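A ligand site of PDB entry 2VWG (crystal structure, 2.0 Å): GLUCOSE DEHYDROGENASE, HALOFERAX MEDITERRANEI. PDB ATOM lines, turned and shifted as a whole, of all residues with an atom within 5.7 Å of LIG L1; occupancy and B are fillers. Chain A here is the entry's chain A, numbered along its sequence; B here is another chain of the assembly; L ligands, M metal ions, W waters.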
ATOM      1  N   ASP A  38      39.703   4.936 -17.244  1.00  0.00           N
ATOM      2  CA  ASP A  38      38.233   4.791 -17.182  1.00  0.00           C
ATOM      3  C   ASP A  38      37.779   3.418 -17.671  1.00  0.00           C
ATOM      4  O   ASP A  38      38.604   2.562 -17.997  1.00  0.00           O
ATOM      5  CB  ASP A  38      37.513   5.941 -17.918  1.00  0.00           C
ATOM      6  CG  ASP A  38      37.572   5.819 -19.438  1.00  0.00           C
ATOM      7  OD1 ASP A  38      38.264   4.929 -19.948  1.00  0.00           O
ATOM      8  OD2 ASP A  38      36.938   6.632 -20.124  1.00  0.00           O
ATOM      9  N   GLY A  39      36.463   3.235 -17.696  1.00  0.00           N
ATOM     10  CA  GLY A  39      35.849   2.005 -18.161  1.00  0.00           C
ATOM     11  C   GLY A  39      36.275   1.601 -19.555  1.00  0.00           C
ATOM     12  O   GLY A  39      36.432   0.428 -19.834  1.00  0.00           O
ATOM     13  N   THR A  40      36.442   2.574 -20.450  1.00  0.00           N
ATOM     14  CA  THR A  40      36.869   2.295 -21.823  1.00  0.00           C
ATOM     15  C   THR A  40      38.254   1.642 -21.835  1.00  0.00           C
ATOM     16  O   THR A  40      38.490   0.704 -22.601  1.00  0.00           O
ATOM     17  CB  THR A  40      36.885   3.566 -22.679  1.00  0.00           C
ATOM     18  OG1 THR A  40      35.572   4.177 -22.661  1.00  0.00           O
ATOM     19  CG2 THR A  40      37.298   3.230 -24.115  1.00  0.00           C
ATOM     20  N   HIS A  63      43.868   7.896 -22.722  1.00  0.00           N
ATOM     21  CA  HIS A  63      43.294   8.907 -23.603  1.00  0.00           C
ATOM     22  C   HIS A  63      42.856  10.164 -22.859  1.00  0.00           C
ATOM     23  O   HIS A  63      42.410  11.118 -23.479  1.00  0.00           O
ATOM     24  CB  HIS A  63      42.145   8.287 -24.408  1.00  0.00           C
ATOM     25  CG  HIS A  63      41.008   7.815 -23.560  1.00  0.00           C
ATOM     26  ND1 HIS A  63      40.967   6.545 -23.024  1.00  0.00           N
ATOM     27  CD2 HIS A  63      39.909   8.462 -23.099  1.00  0.00           C
ATOM     28  CE1 HIS A  63      39.867   6.431 -22.288  1.00  0.00           C
ATOM     29  NE2 HIS A  63      39.215   7.564 -22.327  1.00  0.00           N
ATOM     30  N   ILE A 154      33.238  14.967 -22.942  1.00  0.00           N
ATOM     31  CA  ILE A 154      32.328  13.945 -23.466  1.00  0.00           C
ATOM     32  C   ILE A 154      30.873  14.322 -23.178  1.00  0.00           C
ATOM     33  O   ILE A 154      30.017  14.304 -24.070  1.00  0.00           O
ATOM     34  CB  ILE A 154      32.653  12.529 -22.857  1.00  0.00           C
ATOM     35  CG1 ILE A 154      34.022  12.027 -23.344  1.00  0.00           C
ATOM     36  CG2 ILE A 154      31.540  11.470 -23.167  1.00  0.00           C
ATOM     37  CD1 ILE A 154      34.172  11.964 -24.843  1.00  0.00           C
ATOM     38  N   LEU A 179      22.058   7.116 -15.774  1.00  0.00           N
ATOM     39  CA  LEU A 179      22.147   5.672 -15.657  1.00  0.00           C
ATOM     40  C   LEU A 179      23.603   5.289 -15.551  1.00  0.00           C
ATOM     41  O   LEU A 179      24.361   5.462 -16.516  1.00  0.00           O
ATOM     42  CB  LEU A 179      21.492   4.964 -16.836  1.00  0.00           C
ATOM     43  CG  LEU A 179      20.124   5.467 -17.292  1.00  0.00           C
ATOM     44  CD1 LEU A 179      19.625   4.573 -18.432  1.00  0.00           C
ATOM     45  CD2 LEU A 179      19.131   5.526 -16.137  1.00  0.00           C
ATOM     46  N   GLY A 180      23.990   4.780 -14.396  1.00  0.00           N
ATOM     47  CA  GLY A 180      25.356   4.339 -14.161  1.00  0.00           C
ATOM     48  C   GLY A 180      26.057   5.191 -13.133  1.00  0.00           C
ATOM     49  O   GLY A 180      25.948   6.409 -13.135  1.00  0.00           O
ATOM     50  N   ASN A 181      26.803   4.530 -12.247  1.00  0.00           N
ATOM     51  CA  ASN A 181      27.486   5.182 -11.135  1.00  0.00           C
ATOM     52  C   ASN A 181      28.996   5.014 -11.261  1.00  0.00           C
ATOM     53  O   ASN A 181      29.722   4.947 -10.255  1.00  0.00           O
ATOM     54  CB  ASN A 181      26.984   4.630  -9.786  1.00  0.00           C
ATOM     55  CG  ASN A 181      27.170   3.127  -9.676  1.00  0.00           C
ATOM     56  OD1 ASN A 181      27.019   2.390 -10.657  1.00  0.00           O
ATOM     57  ND2 ASN A 181      27.494   2.655  -8.477  1.00  0.00           N
ATOM     58  N   GLY A 182      29.460   4.931 -12.512  1.00  0.00           N
ATOM     59  CA  GLY A 182      30.881   4.960 -12.799  1.00  0.00           C
ATOM     60  C   GLY A 182      31.366   6.384 -12.783  1.00  0.00           C
ATOM     61  O   GLY A 182      30.594   7.307 -12.499  1.00  0.00           O
ATOM     62  N   SER A 183      32.634   6.578 -13.114  1.00  0.00           N
ATOM     63  CA  SER A 183      33.219   7.907 -13.066  1.00  0.00           C
ATOM     64  C   SER A 183      32.532   8.849 -14.065  1.00  0.00           C
ATOM     65  O   SER A 183      32.320  10.027 -13.752  1.00  0.00           O
ATOM     66  CB  SER A 183      34.728   7.853 -13.321  1.00  0.00           C
ATOM     67  OG  SER A 183      34.993   7.233 -14.559  1.00  0.00           O
ATOM     68  N   LEU A 184      32.153   8.350 -15.243  1.00  0.00           N
ATOM     69  CA  LEU A 184      31.439   9.211 -16.200  1.00  0.00           C
ATOM     70  C   LEU A 184      30.045   9.608 -15.690  1.00  0.00           C
ATOM     71  O   LEU A 184      29.639  10.770 -15.796  1.00  0.00           O
ATOM     72  CB  LEU A 184      31.319   8.543 -17.593  1.00  0.00           C
ATOM     73  CG  LEU A 184      30.724   9.434 -18.700  1.00  0.00           C
ATOM     74  CD1 LEU A 184      31.566  10.689 -18.936  1.00  0.00           C
ATOM     75  CD2 LEU A 184      30.551   8.636 -19.994  1.00  0.00           C
ATOM     76  N   GLY A 185      29.294   8.643 -15.177  1.00  0.00           N
ATOM     77  CA  GLY A 185      27.958   8.911 -14.634  1.00  0.00           C
ATOM     78  C   GLY A 185      27.992   9.899 -13.475  1.00  0.00           C
ATOM     79  O   GLY A 185      27.203  10.843 -13.428  1.00  0.00           O
ATOM     80  N   LEU A 205      21.168   5.871 -11.237  1.00  0.00           N
ATOM     81  CA  LEU A 205      20.975   4.438 -11.176  1.00  0.00           C
ATOM     82  C   LEU A 205      22.284   3.695 -10.970  1.00  0.00           C
ATOM     83  O   LEU A 205      23.289   3.978 -11.647  1.00  0.00           O
ATOM     84  CB  LEU A 205      20.364   3.938 -12.499  1.00  0.00           C
ATOM     85  CG  LEU A 205      19.884   2.476 -12.554  1.00  0.00           C
ATOM     86  CD1 LEU A 205      18.429   2.371 -12.126  1.00  0.00           C
ATOM     87  CD2 LEU A 205      20.056   1.903 -13.940  1.00  0.00           C
ATOM     88  N   GLY A 206      22.268   2.752 -10.048  1.00  0.00           N
ATOM     89  CA  GLY A 206      23.389   1.840  -9.820  1.00  0.00           C
ATOM     90  C   GLY A 206      22.836   0.527  -9.278  1.00  0.00           C
ATOM     91  O   GLY A 206      21.621   0.339  -9.282  1.00  0.00           O
ATOM     92  N   ARG A 207      23.709  -0.361  -8.824  1.00  0.00           N
ATOM     93  CA  ARG A 207      23.288  -1.658  -8.296  1.00  0.00           C
ATOM     94  C   ARG A 207      24.212  -2.100  -7.159  1.00  0.00           C
ATOM     95  O   ARG A 207      24.674  -3.235  -7.147  1.00  0.00           O
ATOM     96  CB  ARG A 207      23.274  -2.704  -9.408  1.00  0.00           C
ATOM     97  CG  ARG A 207      24.563  -2.795 -10.205  1.00  0.00           C
ATOM     98  CD  ARG A 207      24.512  -3.915 -11.232  1.00  0.00           C
ATOM     99  NE  ARG A 207      25.766  -3.982 -11.972  1.00  0.00           N
ATOM    100  CZ  ARG A 207      25.970  -4.705 -13.070  1.00  0.00           C
ATOM    101  NH1 ARG A 207      25.011  -5.442 -13.598  1.00  0.00           N
ATOM    102  NH2 ARG A 207      27.165  -4.677 -13.646  1.00  0.00           N
ATOM    103  N   ARG A 208      24.493  -1.187  -6.225  1.00  0.00           N
ATOM    104  CA  ARG A 208      25.380  -1.437  -5.081  1.00  0.00           C
ATOM    105  C   ARG A 208      24.572  -1.556  -3.797  1.00  0.00           C
ATOM    106  O   ARG A 208      23.516  -0.920  -3.646  1.00  0.00           O
ATOM    107  CB  ARG A 208      26.381  -0.282  -4.881  1.00  0.00           C
ATOM    108  CG  ARG A 208      27.279   0.018  -6.074  1.00  0.00           C
ATOM    109  CD  ARG A 208      28.226  -1.089  -6.356  1.00  0.00           C
ATOM    110  NE  ARG A 208      29.102  -0.807  -7.495  1.00  0.00           N
ATOM    111  CZ  ARG A 208      30.150  -0.004  -7.476  1.00  0.00           C
ATOM    112  NH1 ARG A 208      30.496   0.655  -6.373  1.00  0.00           N
ATOM    113  NH2 ARG A 208      30.878   0.165  -8.574  1.00  0.00           N
ATOM    114  N   SER A 228      18.863  -0.554  -9.432  1.00  0.00           N
ATOM    115  CA  SER A 228      18.236  -1.242 -10.580  1.00  0.00           C
ATOM    116  C   SER A 228      17.771  -2.664 -10.269  1.00  0.00           C
ATOM    117  O   SER A 228      16.904  -3.195 -10.966  1.00  0.00           O
ATOM    118  CB  SER A 228      19.195  -1.270 -11.773  1.00  0.00           C
ATOM    119  OG  SER A 228      20.313  -2.120 -11.551  1.00  0.00           O
ATOM    120  N   GLU A 248      22.576   7.938 -20.427  1.00  0.00           N
ATOM    121  CA  GLU A 248      22.922   6.541 -20.237  1.00  0.00           C
ATOM    122  C   GLU A 248      24.435   6.389 -20.244  1.00  0.00           C
ATOM    123  O   GLU A 248      25.097   6.742 -21.209  1.00  0.00           O
ATOM    124  CB  GLU A 248      22.273   5.671 -21.324  1.00  0.00           C
ATOM    125  CG  GLU A 248      22.717   4.202 -21.311  1.00  0.00           C
ATOM    126  CD  GLU A 248      24.011   3.963 -22.061  1.00  0.00           C
ATOM    127  OE1 GLU A 248      24.188   4.512 -23.176  1.00  0.00           O
ATOM    128  OE2 GLU A 248      24.868   3.234 -21.519  1.00  0.00           O
ATOM    129  N   ALA A 249      24.984   5.842 -19.155  1.00  0.00           N
ATOM    130  CA  ALA A 249      26.416   5.633 -19.012  1.00  0.00           C
ATOM    131  C   ALA A 249      26.714   4.282 -18.337  1.00  0.00           C
ATOM    132  O   ALA A 249      27.638   4.183 -17.529  1.00  0.00           O
ATOM    133  CB  ALA A 249      27.063   6.787 -18.239  1.00  0.00           C
ATOM    134  N   THR A 250      25.935   3.259 -18.708  1.00  0.00           N
ATOM    135  CA  THR A 250      26.148   1.898 -18.210  1.00  0.00           C
ATOM    136  C   THR A 250      26.727   0.954 -19.248  1.00  0.00           C
ATOM    137  O   THR A 250      27.352  -0.036 -18.882  1.00  0.00           O
ATOM    138  CB  THR A 250      24.852   1.254 -17.692  1.00  0.00           C
ATOM    139  OG1 THR A 250      23.902   1.137 -18.756  1.00  0.00           O
ATOM    140  CG2 THR A 250      24.279   2.085 -16.576  1.00  0.00           C
ATOM    141  N   GLY A 251      26.506   1.232 -20.530  1.00  0.00           N
ATOM    142  CA  GLY A 251      26.880   0.281 -21.579  1.00  0.00           C
ATOM    143  C   GLY A 251      26.002  -0.965 -21.619  1.00  0.00           C
ATOM    144  O   GLY A 251      26.326  -1.918 -22.306  1.00  0.00           O
ATOM    145  N   PHE A 252      24.868  -0.936 -20.928  1.00  0.00           N
ATOM    146  CA  PHE A 252      23.940  -2.048 -20.874  1.00  0.00           C
ATOM    147  C   PHE A 252      22.776  -1.829 -21.856  1.00  0.00           C
ATOM    148  O   PHE A 252      21.917  -0.971 -21.628  1.00  0.00           O
ATOM    149  CB  PHE A 252      23.407  -2.164 -19.449  1.00  0.00           C
ATOM    150  CG  PHE A 252      22.559  -3.375 -19.204  1.00  0.00           C
ATOM    151  CD1 PHE A 252      22.967  -4.633 -19.623  1.00  0.00           C
ATOM    152  CD2 PHE A 252      21.365  -3.252 -18.498  1.00  0.00           C
ATOM    153  CE1 PHE A 252      22.172  -5.750 -19.372  1.00  0.00           C
ATOM    154  CE2 PHE A 252      20.578  -4.370 -18.241  1.00  0.00           C
ATOM    155  CZ  PHE A 252      20.981  -5.607 -18.669  1.00  0.00           C
ATOM    156  N   HIS A 255      19.132  -0.752 -21.194  1.00  0.00           N
ATOM    157  CA  HIS A 255      18.921   0.635 -20.780  1.00  0.00           C
ATOM    158  C   HIS A 255      18.666   1.559 -21.955  1.00  0.00           C
ATOM    159  O   HIS A 255      17.921   2.526 -21.836  1.00  0.00           O
ATOM    160  CB  HIS A 255      20.101   1.148 -19.970  1.00  0.00           C
ATOM    161  CG  HIS A 255      20.220   0.528 -18.622  1.00  0.00           C
ATOM    162  ND1 HIS A 255      21.383   0.583 -17.882  1.00  0.00           N
ATOM    163  CD2 HIS A 255      19.336  -0.177 -17.880  1.00  0.00           C
ATOM    164  CE1 HIS A 255      21.198  -0.064 -16.734  1.00  0.00           C
ATOM    165  NE2 HIS A 255      19.963  -0.522 -16.716  1.00  0.00           N
ATOM    166  N   LEU A 271      22.650   8.712 -25.244  1.00  0.00           N
ATOM    167  CA  LEU A 271      23.285   7.405 -25.075  1.00  0.00           C
ATOM    168  C   LEU A 271      24.784   7.548 -25.261  1.00  0.00           C
ATOM    169  O   LEU A 271      25.236   8.074 -26.280  1.00  0.00           O
ATOM    170  CB  LEU A 271      22.716   6.400 -26.080  1.00  0.00           C
ATOM    171  CG  LEU A 271      21.201   6.216 -26.059  1.00  0.00           C
ATOM    172  CD1 LEU A 271      20.792   5.258 -27.184  1.00  0.00           C
ATOM    173  CD2 LEU A 271      20.711   5.718 -24.675  1.00  0.00           C
ATOM    174  N   LEU A 272      25.543   7.083 -24.271  1.00  0.00           N
ATOM    175  CA  LEU A 272      27.024   7.192 -24.287  1.00  0.00           C
ATOM    176  C   LEU A 272      27.741   5.868 -24.137  1.00  0.00           C
ATOM    177  O   LEU A 272      28.940   5.775 -24.404  1.00  0.00           O
ATOM    178  CB  LEU A 272      27.512   8.107 -23.149  1.00  0.00           C
ATOM    179  CG  LEU A 272      27.367   9.634 -23.258  1.00  0.00           C
ATOM    180  CD1 LEU A 272      28.240  10.205 -24.376  1.00  0.00           C
ATOM    181  CD2 LEU A 272      25.911  10.064 -23.391  1.00  0.00           C
ATOM    182  N   GLY A 273      27.026   4.837 -23.682  1.00  0.00           N
ATOM    183  CA  GLY A 273      27.672   3.582 -23.356  1.00  0.00           C
ATOM    184  C   GLY A 273      28.159   2.871 -24.594  1.00  0.00           C
ATOM    185  O   GLY A 273      27.531   2.935 -25.651  1.00  0.00           O
ATOM    186  N   VAL A 274      29.278   2.173 -24.456  1.00  0.00           N
ATOM    187  CA  VAL A 274      29.823   1.333 -25.526  1.00  0.00           C
ATOM    188  C   VAL A 274      29.462  -0.097 -25.136  1.00  0.00           C
ATOM    189  O   VAL A 274      30.055  -0.666 -24.220  1.00  0.00           O
ATOM    190  CB  VAL A 274      31.335   1.492 -25.651  1.00  0.00           C
ATOM    191  CG1 VAL A 274      31.875   0.595 -26.763  1.00  0.00           C
ATOM    192  CG2 VAL A 274      31.682   2.962 -25.915  1.00  0.00           C
ATOM    193  N   PRO A 275      28.454  -0.670 -25.795  1.00  0.00           N
ATOM    194  CA  PRO A 275      27.882  -1.907 -25.319  1.00  0.00           C
ATOM    195  C   PRO A 275      28.533  -3.149 -25.910  1.00  0.00           C
ATOM    196  O   PRO A 275      29.290  -3.059 -26.879  1.00  0.00           O
ATOM    197  CB  PRO A 275      26.435  -1.817 -25.818  1.00  0.00           C
ATOM    198  CG  PRO A 275      26.546  -1.078 -27.057  1.00  0.00           C
ATOM    199  CD  PRO A 275      27.773  -0.210 -27.012  1.00  0.00           C
ATOM    200  N   SER A 301      26.070   9.726 -28.797  1.00  0.00           N
ATOM    201  CA  SER A 301      27.187  10.651 -28.850  1.00  0.00           C
ATOM    202  C   SER A 301      28.496   9.938 -28.504  1.00  0.00           C
ATOM    203  O   SER A 301      28.549   9.137 -27.578  1.00  0.00           O
ATOM    204  CB  SER A 301      26.961  11.810 -27.883  1.00  0.00           C
ATOM    205  OG  SER A 301      27.970  12.803 -28.021  1.00  0.00           O
ATOM    206  N   VAL A 302      29.536  10.243 -29.266  1.00  0.00           N
ATOM    207  CA  VAL A 302      30.854   9.682 -28.998  1.00  0.00           C
ATOM    208  C   VAL A 302      31.913  10.747 -29.221  1.00  0.00           C
ATOM    209  O   VAL A 302      31.756  11.626 -30.084  1.00  0.00           O
ATOM    210  CB  VAL A 302      31.129   8.406 -29.861  1.00  0.00           C
ATOM    211  CG1 VAL A 302      31.261   8.756 -31.361  1.00  0.00           C
ATOM    212  CG2 VAL A 302      32.379   7.666 -29.343  1.00  0.00           C
ATOM    213  N   ASN A 303      32.969  10.698 -28.409  1.00  0.00           N
ATOM    214  CA  ASN A 303      34.124  11.558 -28.585  1.00  0.00           C
ATOM    215  C   ASN A 303      33.717  13.013 -28.292  1.00  0.00           C
ATOM    216  O   ASN A 303      32.670  13.270 -27.686  1.00  0.00           O
ATOM    217  CB  ASN A 303      34.732  11.335 -29.996  1.00  0.00           C
ATOM    218  CG  ASN A 303      36.149  11.879 -30.125  1.00  0.00           C
ATOM    219  OD1 ASN A 303      36.378  12.796 -30.897  1.00  0.00           O
ATOM    220  ND2 ASN A 303      37.101  11.293 -29.394  1.00  0.00           N
ATOM    221  N   ASP A 343      39.982  -2.437  -9.950  1.00  0.00           N
ATOM    222  CA  ASP A 343      38.605  -2.044 -10.099  1.00  0.00           C
ATOM    223  C   ASP A 343      37.746  -2.786  -9.082  1.00  0.00           C
ATOM    224  O   ASP A 343      37.169  -3.834  -9.381  1.00  0.00           O
ATOM    225  CB  ASP A 343      38.123  -2.316 -11.540  1.00  0.00           C
ATOM    226  CG  ASP A 343      36.863  -1.531 -11.892  1.00  0.00           C
ATOM    227  OD1 ASP A 343      36.563  -0.514 -11.230  1.00  0.00           O
ATOM    228  OD2 ASP A 343      36.167  -1.945 -12.854  1.00  0.00           O
ATOM    229  N   ASP A 345      34.702  -1.886  -5.817  1.00  0.00           N
ATOM    230  CA  ASP A 345      33.608  -0.936  -5.588  1.00  0.00           C
ATOM    231  C   ASP A 345      34.047   0.418  -5.037  1.00  0.00           C
ATOM    232  O   ASP A 345      33.361   1.421  -5.243  1.00  0.00           O
ATOM    233  CB  ASP A 345      32.583  -1.543  -4.617  1.00  0.00           C
ATOM    234  CG  ASP A 345      31.834  -2.726  -5.214  1.00  0.00           C
ATOM    235  OD1 ASP A 345      31.877  -2.948  -6.448  1.00  0.00           O
ATOM    236  OD2 ASP A 345      31.182  -3.434  -4.433  1.00  0.00           O
ATOM    237  N   ILE A 348      36.826   4.681  -7.710  1.00  0.00           N
ATOM    238  CA  ILE A 348      35.971   5.454  -8.588  1.00  0.00           C
ATOM    239  C   ILE A 348      36.788   5.943  -9.783  1.00  0.00           C
ATOM    240  O   ILE A 348      36.753   5.309 -10.830  1.00  0.00           O
ATOM    241  CB  ILE A 348      35.235   6.571  -7.831  1.00  0.00           C
ATOM    242  CG1 ILE A 348      34.438   5.962  -6.664  1.00  0.00           C
ATOM    243  CG2 ILE A 348      34.312   7.321  -8.814  1.00  0.00           C
ATOM    244  CD1 ILE A 348      33.680   6.973  -5.813  1.00  0.00           C
ATOM    245  N   VAL B 292      25.407   5.079 -30.593  1.00  0.00           N
ATOM    246  CA  VAL B 292      26.485   5.746 -29.903  1.00  0.00           C
ATOM    247  C   VAL B 292      27.707   5.991 -30.801  1.00  0.00           C
ATOM    248  O   VAL B 292      28.128   7.139 -31.002  1.00  0.00           O
ATOM    249  CB  VAL B 292      26.902   4.963 -28.615  1.00  0.00           C
ATOM    250  CG1 VAL B 292      28.182   5.576 -27.992  1.00  0.00           C
ATOM    251  CG2 VAL B 292      25.748   4.978 -27.613  1.00  0.00           C
HETATM  252  P1  LIG L   1      32.444   2.272 -15.615  1.00  0.00           P
HETATM  253  O1  LIG L   1      33.382   2.862 -14.631  1.00  0.00           O
HETATM  254  O2  LIG L   1      32.560   0.859 -15.968  1.00  0.00           O
HETATM  255  O3  LIG L   1      30.974   2.595 -15.068  1.00  0.00           O
HETATM  256  C1  LIG L   1      29.887   1.833 -15.496  1.00  0.00           C
HETATM  257  C2  LIG L   1      28.949   1.711 -14.322  1.00  0.00           C
HETATM  258  O4  LIG L   1      27.694   1.254 -14.754  1.00  0.00           O
HETATM  259  C3  LIG L   1      29.490   0.741 -13.265  1.00  0.00           C
HETATM  260  O5  LIG L   1      29.686   1.403 -12.035  1.00  0.00           O
HETATM  261  C4  LIG L   1      28.396  -0.307 -13.185  1.00  0.00           C
HETATM  262  O6  LIG L   1      28.153  -0.727 -11.881  1.00  0.00           O
HETATM  263  C5  LIG L   1      27.174   0.408 -13.767  1.00  0.00           C
HETATM  264  N1  LIG L   1      26.214  -0.566 -14.307  1.00  0.00           N
HETATM  265  C6  LIG L   1      26.412  -1.471 -15.318  1.00  0.00           C
HETATM  266  N2  LIG L   1      25.266  -2.167 -15.492  1.00  0.00           N
HETATM  267  C7  LIG L   1      24.357  -1.719 -14.607  1.00  0.00           C
HETATM  268  C8  LIG L   1      23.038  -2.088 -14.350  1.00  0.00           C
HETATM  269  N3  LIG L   1      22.460  -3.048 -15.039  1.00  0.00           N
HETATM  270  N4  LIG L   1      22.354  -1.430 -13.361  1.00  0.00           N
HETATM  271  C9  LIG L   1      22.945  -0.406 -12.638  1.00  0.00           C
HETATM  272  N5  LIG L   1      24.253  -0.057 -12.899  1.00  0.00           N
HETATM  273  C10 LIG L   1      24.934  -0.701 -13.868  1.00  0.00           C
HETATM  274  O7  LIG L   1      32.532   3.120 -16.974  1.00  0.00           O
HETATM  275  P2  LIG L   1      32.701   4.702 -17.181  1.00  0.00           P
HETATM  276  O8  LIG L   1      31.908   5.473 -16.182  1.00  0.00           O
HETATM  277  O9  LIG L   1      34.126   5.040 -17.378  1.00  0.00           O
HETATM  278  O10 LIG L   1      31.938   4.778 -18.600  1.00  0.00           O
HETATM  279  C11 LIG L   1      30.595   4.355 -18.684  1.00  0.00           C
HETATM  280  C12 LIG L   1      30.281   3.893 -20.102  1.00  0.00           C
HETATM  281  O11 LIG L   1      30.432   4.979 -21.003  1.00  0.00           O
HETATM  282  C13 LIG L   1      31.208   2.789 -20.605  1.00  0.00           C
HETATM  283  O12 LIG L   1      30.446   1.933 -21.441  1.00  0.00           O
HETATM  284  C14 LIG L   1      32.225   3.542 -21.421  1.00  0.00           C
HETATM  285  O13 LIG L   1      32.828   2.747 -22.387  1.00  0.00           O
HETATM  286  C15 LIG L   1      31.328   4.626 -22.034  1.00  0.00           C
HETATM  287  N6  LIG L   1      32.026   5.834 -22.488  1.00  0.00           N
HETATM  288  C16 LIG L   1      31.682   6.327 -23.709  1.00  0.00           C
HETATM  289  C17 LIG L   1      32.247   7.484 -24.181  1.00  0.00           C
HETATM  290  C18 LIG L   1      31.688   8.104 -25.421  1.00  0.00           C
HETATM  291  O14 LIG L   1      32.517   8.934 -26.139  1.00  0.00           O
HETATM  292  N7  LIG L   1      30.448   7.793 -25.815  1.00  0.00           N
HETATM  293  C19 LIG L   1      33.205   8.140 -23.428  1.00  0.00           C
HETATM  294  C20 LIG L   1      33.541   7.634 -22.170  1.00  0.00           C
HETATM  295  C21 LIG L   1      32.939   6.473 -21.701  1.00  0.00           C
HETATM  296  P3  LIG L   1      28.943  -1.981 -11.217  1.00  0.00           P
HETATM  297  O15 LIG L   1      30.320  -1.522 -10.911  1.00  0.00           O
HETATM  298  O16 LIG L   1      28.961  -3.157 -12.128  1.00  0.00           O
HETATM  299  O17 LIG L   1      28.169  -2.228  -9.934  1.00  0.00           O
HETATM  300  C1  LG2 L   2      36.153   7.126 -24.719  1.00  0.00           C
HETATM  301  C2  LG2 L   2      36.752   8.435 -25.085  1.00  0.00           C
HETATM  302  O1  LG2 L   2      35.571   6.272 -25.686  1.00  0.00           O
HETATM  303  O2  LG2 L   2      36.191   6.751 -23.552  1.00  0.00           O
HETATM  304  O3  LG2 L   2      36.474   9.375 -24.072  1.00  0.00           O
HETATM  305  C3  LG2 L   2      36.274   8.976 -26.422  1.00  0.00           C
HETATM  306  O4  LG2 L   2      37.202   9.949 -26.880  1.00  0.00           O
HETATM  307  C4  LG2 L   2      36.168   7.875 -27.461  1.00  0.00           C
HETATM  308  O5  LG2 L   2      35.677   8.460 -28.646  1.00  0.00           O
HETATM  309  C5  LG2 L   2      35.208   6.791 -26.958  1.00  0.00           C
HETATM  310  C6  LG2 L   2      35.101   5.634 -27.955  1.00  0.00           C
HETATM  311  O6  LG2 L   2      36.354   5.007 -28.087  1.00  0.00           O
HETATM  312 ZN    ZN M   1      37.902   8.354 -20.823  1.00  0.00          ZN
HETATM  313  O   HOH W   1      29.179   5.494 -15.413  1.00  0.00           O
HETATM  314  O   HOH W   2      34.343   4.004 -11.952  1.00  0.00           O
HETATM  315  O   HOH W   3      34.661   7.579 -18.845  1.00  0.00           O
HETATM  316  O   HOH W   4      26.474  -0.100  -9.510  1.00  0.00           O
HETATM  317  O   HOH W   5      27.854  -4.484  -8.657  1.00  0.00           O
HETATM  318  O   HOH W   6      19.194  -3.431 -14.897  1.00  0.00           O
HETATM  319  O   HOH W   7      32.582   1.705 -11.972  1.00  0.00           O
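Merely in contact with LIG L1: Ala 249 (3.2 Å), Gly 182 (3.3 Å), Val 302 (3.4 Å), Gly 206 (3.5 Å), Asp 38 (3.5 Å), His 255 (3.6 Å), Phe 252 (3.6 Å), Ile 154 (3.7 Å), Gly 273 (3.8 Å), Thr 250 (3.8 Å), Val 292 of chain B (3.8 Å), Gly 180 (3.9 Å), Leu 205 (3.9 Å) and Gly 251 (3.9 Å). Hydrophobic or aromatic side chains that line LIG L1: Ile 154, Leu 184, Leu 205, Phe 252, His 255, Leu 272, Val 274, Val 302 and Val 292 of chain B. Within 4 Å of LIG L1: Asp 38, Gly 39, Thr 40, Ile 154, Gly 180, Asn 181, Gly 182, Ser 183, Leu 184, Leu 205, Gly 206, Arg 207, Arg 208, Ser 228, Ala 249, Thr 250, Gly 251, Phe 252, His 255, Leu 272, Gly 273, Val 274, Ser 301, Val 302, Asn 303 and Val 292 of chain B. The nearest printed residue that does not touch LIG L1 is Gly 185 (4.2 Å).
The side-chain hydroxyl (OG1) of Thr 250 lies close to the backbone NH (N) of Phe 252, 3.2 Å away. The backbone NH (N) of Thr 250 lies close to the backbone carbonyl oxygen (O) of Leu 179. N of Ser 228 is in hydrogen-bond range of O of Gly 206, at 2.9 Å. N of Gly 251 is in hydrogen-bond range of OE2 of Glu 248, at 2.8 Å. A ring nitrogen (ND1) of His 255 lies within hydrogen-bond range of the side-chain hydroxyl (OG1) of Thr 250 (2.7 Å). The backbone NH (N) of Thr 40 sits at hydrogen-bond distance from the side-chain carboxylate (OD1) of Asp 38, at 3.0 Å. The backbone NH of Ser 301 sits at hydrogen-bond distance from the backbone carbonyl oxygen of Leu 271 (3.1 Å). The backbone NH (N) of Ala 249 sits at hydrogen-bond distance from the backbone carbonyl oxygen (O) of Leu 179, 2.7 Å away.
N of Asn 303 is in hydrogen-bond range of O14 of LIG L1 (2.9 Å). The side-chain hydroxyl (OG) of Ser 228 is in hydrogen-bond range of a nitrogen (N4) of LIG L1. O15 of LIG L1 lies within salt-bridge range of NH2 of Arg 208, 2.9 Å away. The side-chain amide nitrogen (ND2) of Asn 303 lies within hydrogen-bond range of an oxygen (O4) of LG2 L2 (2.9 Å). N of Ser 183 is in hydrogen-bond range of O8 of LIG L1. N of Leu 184 is in hydrogen-bond range of O8 of LIG L1. NE2 of His 63 sits close to O2 of LG2 L2 (3.4 Å). The side-chain hydroxyl (OG1) of Thr 40 lies within hydrogen-bond range of an oxygen (O2) of LG2 L2 (2.8 Å). O of Leu 272 sits close to N7 of LIG L1. The guanidinium group (NH2) of Arg 207 lies within salt-bridge range of an oxygen (O16) of LIG L1, at 2.8 Å. The side-chain amide oxygen (OD1) of Asn 181 lies within hydrogen-bond range of an oxygen (O5) of LIG L1, at 3.2 Å. O of Ser 301 sits at hydrogen-bond distance from N7 of LIG L1. N of Gly 39 sits at hydrogen-bond distance from O9 of LIG L1 (3.0 Å). O13 of LIG L1 sits at hydrogen-bond distance from OG1 of Thr 40 (3.1 Å). N of Val 274 is in hydrogen-bond range of O12 of LIG L1 (3.2 Å).
Water W4 lies within hydrogen-bond range of O17 of LIG L1 (2.8 Å), OD1 of Asn 181 (2.8 Å), N of Arg 207 (2.9 Å) and NE of Arg 208 (3.4 Å). Water W1 lies within hydrogen-bond range of O8 of LIG L1 (2.8 Å), O of Ala 249 (2.9 Å), N of Gly 182 (3.0 Å) and N of Gly 185 (3.2 Å). Water W2 lies within hydrogen-bond range of the backbone carbonyl oxygen of Ile 348 (3.0 Å), an oxygen (O1) of LIG L1 (3.1 Å) and the backbone NH of Ser 183 (3.3 Å).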
